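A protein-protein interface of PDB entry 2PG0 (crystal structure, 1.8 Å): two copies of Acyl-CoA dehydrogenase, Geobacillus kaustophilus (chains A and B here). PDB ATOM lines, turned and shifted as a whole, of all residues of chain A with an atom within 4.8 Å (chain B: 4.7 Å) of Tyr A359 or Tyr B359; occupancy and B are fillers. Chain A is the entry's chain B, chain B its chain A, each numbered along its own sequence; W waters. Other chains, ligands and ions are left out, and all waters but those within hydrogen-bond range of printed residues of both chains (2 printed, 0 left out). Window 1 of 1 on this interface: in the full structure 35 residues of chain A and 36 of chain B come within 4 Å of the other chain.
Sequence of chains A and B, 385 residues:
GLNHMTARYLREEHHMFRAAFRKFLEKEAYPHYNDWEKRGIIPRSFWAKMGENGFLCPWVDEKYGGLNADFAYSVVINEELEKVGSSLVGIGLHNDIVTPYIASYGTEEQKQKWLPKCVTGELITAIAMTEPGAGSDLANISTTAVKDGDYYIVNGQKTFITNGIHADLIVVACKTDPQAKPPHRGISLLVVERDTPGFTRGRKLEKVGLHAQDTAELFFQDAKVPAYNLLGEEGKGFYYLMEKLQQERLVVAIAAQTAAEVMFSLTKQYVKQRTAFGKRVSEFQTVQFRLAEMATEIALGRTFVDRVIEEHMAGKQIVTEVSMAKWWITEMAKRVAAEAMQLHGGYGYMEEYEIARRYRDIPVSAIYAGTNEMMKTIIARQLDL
Met A341 touches Pro B363, and with the chains exchanged Pro A363 touches Met B341.
Tyr B359 touches its own counterpart, Tyr A359.
Tyr A359 touches Pro B363, and with the chains exchanged Pro A363 touches Tyr B359.
Positions printed for both chains: 263, 337, 338, 341, 355, 356, 357, 358, 359, 360, 361, 362 and 363.
Met A341 touches Pro B363.
OH of Tyr A359 touches OH of Tyr B359 (3.9 Å).
OH of Tyr A359 touches CG of Pro B363 (3.6 Å).
Pro A363 touches Met B341.
Pro A363 touches Tyr B359.
Water W1 bridges the side-chain hydroxyl (OH) of Tyr A359 (2.7 Å) and the backbone carbonyl oxygen (O) of Tyr B359 (2.8 Å).
Water W2 lies within hydrogen-bond range of the side-chain hydroxyl of Tyr B359 (2.8 Å) and the backbone carbonyl oxygen of Tyr A359 (2.8 Å).
Along chain A the printed residues that touch a printed residue of chain B span positions 341 to 363.
Printed residues of chain B that touch a printed residue of chain A: Met B341, Tyr B359 and Pro B363.
Hydrophobic or aromatic side chains of chain B that line the printed part of chain A: Met B341, Tyr B359 and Pro B363.
Among the printed residues, 5 pairs touch across the chains.
Among the printed residues, no Asp or Glu carboxylate lies within 4 Å of a Lys or Arg side-chain nitrogen of the other chain.
Of the printed residues of chain B, Met A341 touches Pro B363.
Ile A362 touches none of the printed residues of chain B.
Printed residues of chain B within 4 Å of Pro A363: Met B341 and Tyr B359.
Printed residues of chain A within 4 Å of Met B341: Pro A363 (3.6 Å).
Tyr B359 touches two residues of chain A.
Of the printed residues of chain A, Pro B363 touches Met A341 and Tyr A359.
The nearest printed residue of chain B that does not touch Met A341 is Arg B360 (6.1 Å).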
ATOM      1  N   MET A 263       1.577  24.923  16.416  1.00  0.00           N
ATOM      2  CA  MET A 263       1.115  23.984  17.429  1.00  0.00           C
ATOM      3  C   MET A 263      -0.380  24.126  17.727  1.00  0.00           C
ATOM      4  O   MET A 263      -1.072  23.123  17.954  1.00  0.00           O
ATOM      5  CB  MET A 263       1.937  24.106  18.726  1.00  0.00           C
ATOM      6  CG  MET A 263       3.358  23.523  18.604  1.00  0.00           C
ATOM      7  SD  MET A 263       4.349  23.488  20.149  1.00  0.00           S
ATOM      8  CE  MET A 263       4.755  25.228  20.334  1.00  0.00           C
ATOM      9  N   ALA A 337       2.511  24.527  23.857  1.00  0.00           N
ATOM     10  CA  ALA A 337       3.073  23.189  23.710  1.00  0.00           C
ATOM     11  C   ALA A 337       2.526  22.211  24.755  1.00  0.00           C
ATOM     12  O   ALA A 337       2.184  21.073  24.421  1.00  0.00           O
ATOM     13  CB  ALA A 337       4.600  23.237  23.782  1.00  0.00           C
ATOM     14  N   ALA A 338       2.469  22.645  26.014  1.00  0.00           N
ATOM     15  CA  ALA A 338       1.994  21.788  27.106  1.00  0.00           C
ATOM     16  C   ALA A 338       0.513  21.430  26.920  1.00  0.00           C
ATOM     17  O   ALA A 338       0.104  20.280  27.120  1.00  0.00           O
ATOM     18  CB  ALA A 338       2.209  22.469  28.451  1.00  0.00           C
ATOM     19  N   MET A 341       0.302  18.837  23.821  1.00  0.00           N
ATOM     20  CA  MET A 341       0.583  17.432  24.155  1.00  0.00           C
ATOM     21  C   MET A 341      -0.614  16.824  24.892  1.00  0.00           C
ATOM     22  O   MET A 341      -1.107  15.768  24.506  1.00  0.00           O
ATOM     23  CB  MET A 341       1.875  17.243  24.976  1.00  0.00           C
ATOM     24  CG  MET A 341       2.238  15.736  25.224  1.00  0.00           C
ATOM     25  SD  MET A 341       3.610  15.601  26.406  1.00  0.00           S
ATOM     26  CE  MET A 341       4.931  15.736  25.204  1.00  0.00           C
ATOM     27  N   ILE A 355       3.557  16.912  16.734  1.00  0.00           N
ATOM     28  CA  ILE A 355       3.468  17.697  17.965  1.00  0.00           C
ATOM     29  C   ILE A 355       4.540  17.306  19.000  1.00  0.00           C
ATOM     30  O   ILE A 355       4.998  18.158  19.768  1.00  0.00           O
ATOM     31  CB  ILE A 355       2.037  17.671  18.597  1.00  0.00           C
ATOM     32  CG1 ILE A 355       1.874  18.800  19.619  1.00  0.00           C
ATOM     33  CG2 ILE A 355       1.715  16.313  19.237  1.00  0.00           C
ATOM     34  CD1 ILE A 355       1.946  20.202  19.010  1.00  0.00           C
ATOM     35  N   ALA A 356       4.947  16.035  18.995  1.00  0.00           N
ATOM     36  CA  ALA A 356       5.986  15.559  19.920  1.00  0.00           C
ATOM     37  C   ALA A 356       7.289  16.320  19.696  1.00  0.00           C
ATOM     38  O   ALA A 356       7.914  16.790  20.649  1.00  0.00           O
ATOM     39  CB  ALA A 356       6.204  14.062  19.764  1.00  0.00           C
ATOM     40  N   ARG A 357       7.697  16.428  18.434  1.00  0.00           N
ATOM     41  CA  ARG A 357       8.902  17.166  18.057  1.00  0.00           C
ATOM     42  C   ARG A 357       8.759  18.667  18.335  1.00  0.00           C
ATOM     43  O   ARG A 357       9.670  19.282  18.872  1.00  0.00           O
ATOM     44  CB  ARG A 357       9.264  16.898  16.586  1.00  0.00           C
ATOM     45  CG  ARG A 357      10.410  17.752  16.034  1.00  0.00           C
ATOM     46  CD  ARG A 357       9.889  18.879  15.147  1.00  0.00           C
ATOM     47  NE  ARG A 357       9.294  18.362  13.915  1.00  0.00           N
ATOM     48  CZ  ARG A 357       8.941  19.112  12.870  1.00  0.00           C
ATOM     49  NH1 ARG A 357       9.099  20.435  12.895  1.00  0.00           N
ATOM     50  NH2 ARG A 357       8.420  18.526  11.789  1.00  0.00           N
ATOM     51  N   ARG A 358       7.616  19.251  17.982  1.00  0.00           N
ATOM     52  CA  ARG A 358       7.363  20.663  18.285  1.00  0.00           C
ATOM     53  C   ARG A 358       7.499  20.924  19.795  1.00  0.00           C
ATOM     54  O   ARG A 358       8.088  21.930  20.217  1.00  0.00           O
ATOM     55  CB  ARG A 358       5.971  21.084  17.801  1.00  0.00           C
ATOM     56  CG  ARG A 358       5.718  20.841  16.305  1.00  0.00           C
ATOM     57  CD  ARG A 358       6.159  21.999  15.441  1.00  0.00           C
ATOM     58  NE  ARG A 358       5.945  21.730  14.011  1.00  0.00           N
ATOM     59  CZ  ARG A 358       6.439  22.480  13.032  1.00  0.00           C
ATOM     60  NH1 ARG A 358       7.167  23.549  13.318  1.00  0.00           N
ATOM     61  NH2 ARG A 358       6.201  22.166  11.763  1.00  0.00           N
ATOM     62  N   TYR A 359       6.956  20.009  20.593  1.00  0.00           N
ATOM     63  CA  TYR A 359       7.007  20.099  22.058  1.00  0.00           C
ATOM     64  C   TYR A 359       8.449  20.121  22.573  1.00  0.00           C
ATOM     65  O   TYR A 359       8.796  20.952  23.420  1.00  0.00           O
ATOM     66  CB  TYR A 359       6.239  18.934  22.695  1.00  0.00           C
ATOM     67  CG  TYR A 359       6.298  18.897  24.210  1.00  0.00           C
ATOM     68  CD1 TYR A 359       5.281  19.464  24.973  1.00  0.00           C
ATOM     69  CD2 TYR A 359       7.374  18.291  24.879  1.00  0.00           C
ATOM     70  CE1 TYR A 359       5.324  19.439  26.363  1.00  0.00           C
ATOM     71  CE2 TYR A 359       7.427  18.250  26.269  1.00  0.00           C
ATOM     72  CZ  TYR A 359       6.396  18.825  27.008  1.00  0.00           C
ATOM     73  OH  TYR A 359       6.431  18.808  28.385  1.00  0.00           O
ATOM     74  N   ARG A 360       9.277  19.204  22.070  1.00  0.00           N
ATOM     75  CA  ARG A 360      10.696  19.126  22.472  1.00  0.00           C
ATOM     76  C   ARG A 360      11.507  20.329  21.996  1.00  0.00           C
ATOM     77  O   ARG A 360      12.481  20.719  22.640  1.00  0.00           O
ATOM     78  CB  ARG A 360      11.348  17.840  21.965  1.00  0.00           C
ATOM     79  CG  ARG A 360      10.869  16.550  22.650  1.00  0.00           C
ATOM     80  CD  ARG A 360      11.709  15.351  22.240  1.00  0.00           C
ATOM     81  NE  ARG A 360      11.385  14.919  20.883  1.00  0.00           N
ATOM     82  CZ  ARG A 360      12.079  15.247  19.797  1.00  0.00           C
ATOM     83  NH1 ARG A 360      13.171  16.005  19.892  1.00  0.00           N
ATOM     84  NH2 ARG A 360      11.679  14.809  18.613  1.00  0.00           N
ATOM     85  N   ASP A 361      11.097  20.919  20.874  1.00  0.00           N
ATOM     86  CA  ASP A 361      11.844  22.020  20.274  1.00  0.00           C
ATOM     87  C   ASP A 361      11.657  23.347  21.006  1.00  0.00           C
ATOM     88  O   ASP A 361      12.596  24.150  21.099  1.00  0.00           O
ATOM     89  CB  ASP A 361      11.475  22.171  18.786  1.00  0.00           C
ATOM     90  CG  ASP A 361      12.119  21.097  17.903  1.00  0.00           C
ATOM     91  OD1 ASP A 361      12.847  20.216  18.424  1.00  0.00           O
ATOM     92  OD2 ASP A 361      11.885  21.144  16.679  1.00  0.00           O
ATOM     93  N   ILE A 362      10.461  23.580  21.549  1.00  0.00           N
ATOM     94  CA  ILE A 362      10.111  24.932  22.012  1.00  0.00           C
ATOM     95  C   ILE A 362      10.823  25.469  23.284  1.00  0.00           C
ATOM     96  O   ILE A 362      11.150  26.659  23.326  1.00  0.00           O
ATOM     97  CB  ILE A 362       8.558  25.145  22.094  1.00  0.00           C
ATOM     98  CG1 ILE A 362       8.192  26.632  22.273  1.00  0.00           C
ATOM     99  CG2 ILE A 362       7.937  24.296  23.196  1.00  0.00           C
ATOM    100  CD1 ILE A 362       8.717  27.546  21.160  1.00  0.00           C
ATOM    101  N   PRO A 363      11.085  24.610  24.302  1.00  0.00           N
ATOM    102  CA  PRO A 363      11.459  25.242  25.587  1.00  0.00           C
ATOM    103  C   PRO A 363      12.802  25.975  25.588  1.00  0.00           C
ATOM    104  O   PRO A 363      13.010  26.874  26.406  1.00  0.00           O
ATOM    105  CB  PRO A 363      11.463  24.082  26.594  1.00  0.00           C
ATOM    106  CG  PRO A 363      11.477  22.836  25.802  1.00  0.00           C
ATOM    107  CD  PRO A 363      11.056  23.139  24.385  1.00  0.00           C
ATOM    108  N   MET B 263      13.668  15.999  40.845  1.00  0.00           N
ATOM    109  CA  MET B 263      13.955  17.160  40.005  1.00  0.00           C
ATOM    110  C   MET B 263      14.292  18.410  40.828  1.00  0.00           C
ATOM    111  O   MET B 263      15.169  19.200  40.443  1.00  0.00           O
ATOM    112  CB  MET B 263      12.800  17.414  39.020  1.00  0.00           C
ATOM    113  CG  MET B 263      12.805  16.431  37.844  1.00  0.00           C
ATOM    114  SD  MET B 263      11.541  16.738  36.558  1.00  0.00           S
ATOM    115  CE  MET B 263      10.061  16.280  37.460  1.00  0.00           C
ATOM    116  N   ALA B 337       9.331  20.388  36.546  1.00  0.00           N
ATOM    117  CA  ALA B 337      10.217  20.065  35.436  1.00  0.00           C
ATOM    118  C   ALA B 337      10.533  21.295  34.578  1.00  0.00           C
ATOM    119  O   ALA B 337      11.684  21.507  34.203  1.00  0.00           O
ATOM    120  CB  ALA B 337       9.618  18.941  34.585  1.00  0.00           C
ATOM    121  N   ALA B 338       9.512  22.108  34.292  1.00  0.00           N
ATOM    122  CA  ALA B 338       9.679  23.329  33.500  1.00  0.00           C
ATOM    123  C   ALA B 338      10.597  24.339  34.192  1.00  0.00           C
ATOM    124  O   ALA B 338      11.453  24.957  33.547  1.00  0.00           O
ATOM    125  CB  ALA B 338       8.312  23.968  33.189  1.00  0.00           C
ATOM    126  N   MET B 341      14.323  22.788  34.111  1.00  0.00           N
ATOM    127  CA  MET B 341      15.027  23.004  32.843  1.00  0.00           C
ATOM    128  C   MET B 341      15.520  24.449  32.756  1.00  0.00           C
ATOM    129  O   MET B 341      16.702  24.683  32.496  1.00  0.00           O
ATOM    130  CB  MET B 341      14.185  22.648  31.604  1.00  0.00           C
ATOM    131  CG  MET B 341      14.997  22.780  30.268  1.00  0.00           C
ATOM    132  SD  MET B 341      13.991  22.662  28.762  1.00  0.00           S
ATOM    133  CE  MET B 341      13.988  20.876  28.654  1.00  0.00           C
ATOM    134  N   ILE B 355      18.537  16.190  34.138  1.00  0.00           N
ATOM    135  CA  ILE B 355      17.276  16.944  34.092  1.00  0.00           C
ATOM    136  C   ILE B 355      16.565  16.887  32.735  1.00  0.00           C
ATOM    137  O   ILE B 355      15.335  16.901  32.693  1.00  0.00           O
ATOM    138  CB  ILE B 355      17.414  18.414  34.600  1.00  0.00           C
ATOM    139  CG1 ILE B 355      16.036  19.004  34.926  1.00  0.00           C
ATOM    140  CG2 ILE B 355      18.174  19.292  33.614  1.00  0.00           C
ATOM    141  CD1 ILE B 355      15.270  18.213  35.995  1.00  0.00           C
ATOM    142  N   ALA B 356      17.327  16.810  31.642  1.00  0.00           N
ATOM    143  CA  ALA B 356      16.736  16.731  30.300  1.00  0.00           C
ATOM    144  C   ALA B 356      15.805  15.520  30.189  1.00  0.00           C
ATOM    145  O   ALA B 356      14.661  15.632  29.724  1.00  0.00           O
ATOM    146  CB  ALA B 356      17.826  16.677  29.233  1.00  0.00           C
ATOM    147  N   ARG B 357      16.310  14.368  30.626  1.00  0.00           N
ATOM    148  CA  ARG B 357      15.565  13.113  30.606  1.00  0.00           C
ATOM    149  C   ARG B 357      14.356  13.148  31.546  1.00  0.00           C
ATOM    150  O   ARG B 357      13.258  12.720  31.174  1.00  0.00           O
ATOM    151  CB  ARG B 357      16.509  11.994  31.008  1.00  0.00           C
ATOM    152  CG  ARG B 357      15.957  10.622  30.999  1.00  0.00           C
ATOM    153  CD  ARG B 357      16.880   9.821  31.895  1.00  0.00           C
ATOM    154  NE  ARG B 357      16.250   9.648  33.171  1.00  0.00           N
ATOM    155  CZ  ARG B 357      16.839   9.288  34.304  1.00  0.00           C
ATOM    156  NH1 ARG B 357      18.159   9.088  34.402  1.00  0.00           N
ATOM    157  NH2 ARG B 357      16.063   9.142  35.355  1.00  0.00           N
ATOM    158  N   ARG B 358      14.558  13.667  32.760  1.00  0.00           N
ATOM    159  CA  ARG B 358      13.466  13.814  33.728  1.00  0.00           C
ATOM    160  C   ARG B 358      12.346  14.670  33.130  1.00  0.00           C
ATOM    161  O   ARG B 358      11.169  14.338  33.266  1.00  0.00           O
ATOM    162  CB  ARG B 358      13.971  14.431  35.038  1.00  0.00           C
ATOM    163  CG  ARG B 358      15.117  13.652  35.713  1.00  0.00           C
ATOM    164  CD  ARG B 358      14.598  12.508  36.547  1.00  0.00           C
ATOM    165  NE  ARG B 358      15.675  11.810  37.258  1.00  0.00           N
ATOM    166  CZ  ARG B 358      15.520  10.670  37.926  1.00  0.00           C
ATOM    167  NH1 ARG B 358      14.328  10.071  37.987  1.00  0.00           N
ATOM    168  NH2 ARG B 358      16.570  10.120  38.532  1.00  0.00           N
ATOM    169  N   TYR B 359      12.733  15.751  32.450  1.00  0.00           N
ATOM    170  CA  TYR B 359      11.785  16.663  31.793  1.00  0.00           C
ATOM    171  C   TYR B 359      10.964  15.958  30.706  1.00  0.00           C
ATOM    172  O   TYR B 359       9.747  16.130  30.638  1.00  0.00           O
ATOM    173  CB  TYR B 359      12.526  17.877  31.212  1.00  0.00           C
ATOM    174  CG  TYR B 359      11.649  18.834  30.422  1.00  0.00           C
ATOM    175  CD1 TYR B 359      11.124  19.981  31.028  1.00  0.00           C
ATOM    176  CD2 TYR B 359      11.368  18.606  29.075  1.00  0.00           C
ATOM    177  CE1 TYR B 359      10.331  20.874  30.311  1.00  0.00           C
ATOM    178  CE2 TYR B 359      10.580  19.488  28.345  1.00  0.00           C
ATOM    179  CZ  TYR B 359      10.059  20.618  28.972  1.00  0.00           C
ATOM    180  OH  TYR B 359       9.280  21.505  28.263  1.00  0.00           O
ATOM    181  N   ARG B 360      11.632  15.174  29.860  1.00  0.00           N
ATOM    182  CA  ARG B 360      10.945  14.425  28.795  1.00  0.00           C
ATOM    183  C   ARG B 360      10.035  13.327  29.345  1.00  0.00           C
ATOM    184  O   ARG B 360       9.034  12.983  28.720  1.00  0.00           O
ATOM    185  CB  ARG B 360      11.952  13.812  27.813  1.00  0.00           C
ATOM    186  CG  ARG B 360      12.624  14.826  26.874  1.00  0.00           C
ATOM    187  CD  ARG B 360      13.455  14.144  25.795  1.00  0.00           C
ATOM    188  NE  ARG B 360      14.656  13.521  26.355  1.00  0.00           N
ATOM    189  CZ  ARG B 360      14.755  12.239  26.691  1.00  0.00           C
ATOM    190  NH1 ARG B 360      13.724  11.417  26.523  1.00  0.00           N
ATOM    191  NH2 ARG B 360      15.895  11.780  27.203  1.00  0.00           N
ATOM    192  N   ASP B 361      10.386  12.791  30.512  1.00  0.00           N
ATOM    193  CA  ASP B 361       9.671  11.650  31.101  1.00  0.00           C
ATOM    194  C   ASP B 361       8.359  12.043  31.788  1.00  0.00           C
ATOM    195  O   ASP B 361       7.383  11.289  31.769  1.00  0.00           O
ATOM    196  CB  ASP B 361      10.577  10.894  32.090  1.00  0.00           C
ATOM    197  CG  ASP B 361      11.635  10.029  31.390  1.00  0.00           C
ATOM    198  OD1 ASP B 361      11.649   9.994  30.142  1.00  0.00           O
ATOM    199  OD2 ASP B 361      12.451   9.372  32.095  1.00  0.00           O
ATOM    200  N   ILE B 362       8.330  13.234  32.374  1.00  0.00           N
ATOM    201  CA  ILE B 362       7.213  13.607  33.243  1.00  0.00           C
ATOM    202  C   ILE B 362       5.834  13.846  32.589  1.00  0.00           C
ATOM    203  O   ILE B 362       4.828  13.467  33.182  1.00  0.00           O
ATOM    204  CB  ILE B 362       7.586  14.774  34.222  1.00  0.00           C
ATOM    205  CG1 ILE B 362       6.565  14.880  35.372  1.00  0.00           C
ATOM    206  CG2 ILE B 362       7.798  16.106  33.476  1.00  0.00           C
ATOM    207  CD1 ILE B 362       6.544  13.640  36.278  1.00  0.00           C
ATOM    208  N   PRO B 363       5.776  14.469  31.390  1.00  0.00           N
ATOM    209  CA  PRO B 363       4.452  14.990  30.997  1.00  0.00           C
ATOM    210  C   PRO B 363       3.394  13.926  30.697  1.00  0.00           C
ATOM    211  O   PRO B 363       2.181  14.201  30.796  1.00  0.00           O
ATOM    212  CB  PRO B 363       4.757  15.857  29.772  1.00  0.00           C
ATOM    213  CG  PRO B 363       6.015  15.324  29.216  1.00  0.00           C
ATOM    214  CD  PRO B 363       6.801  14.744  30.364  1.00  0.00           C
HETATM  215  O   HOH W   1       7.825  18.183  30.633  1.00  0.00           O
HETATM  216  O   HOH W   2       7.928  21.915  25.893  1.00  0.00           O
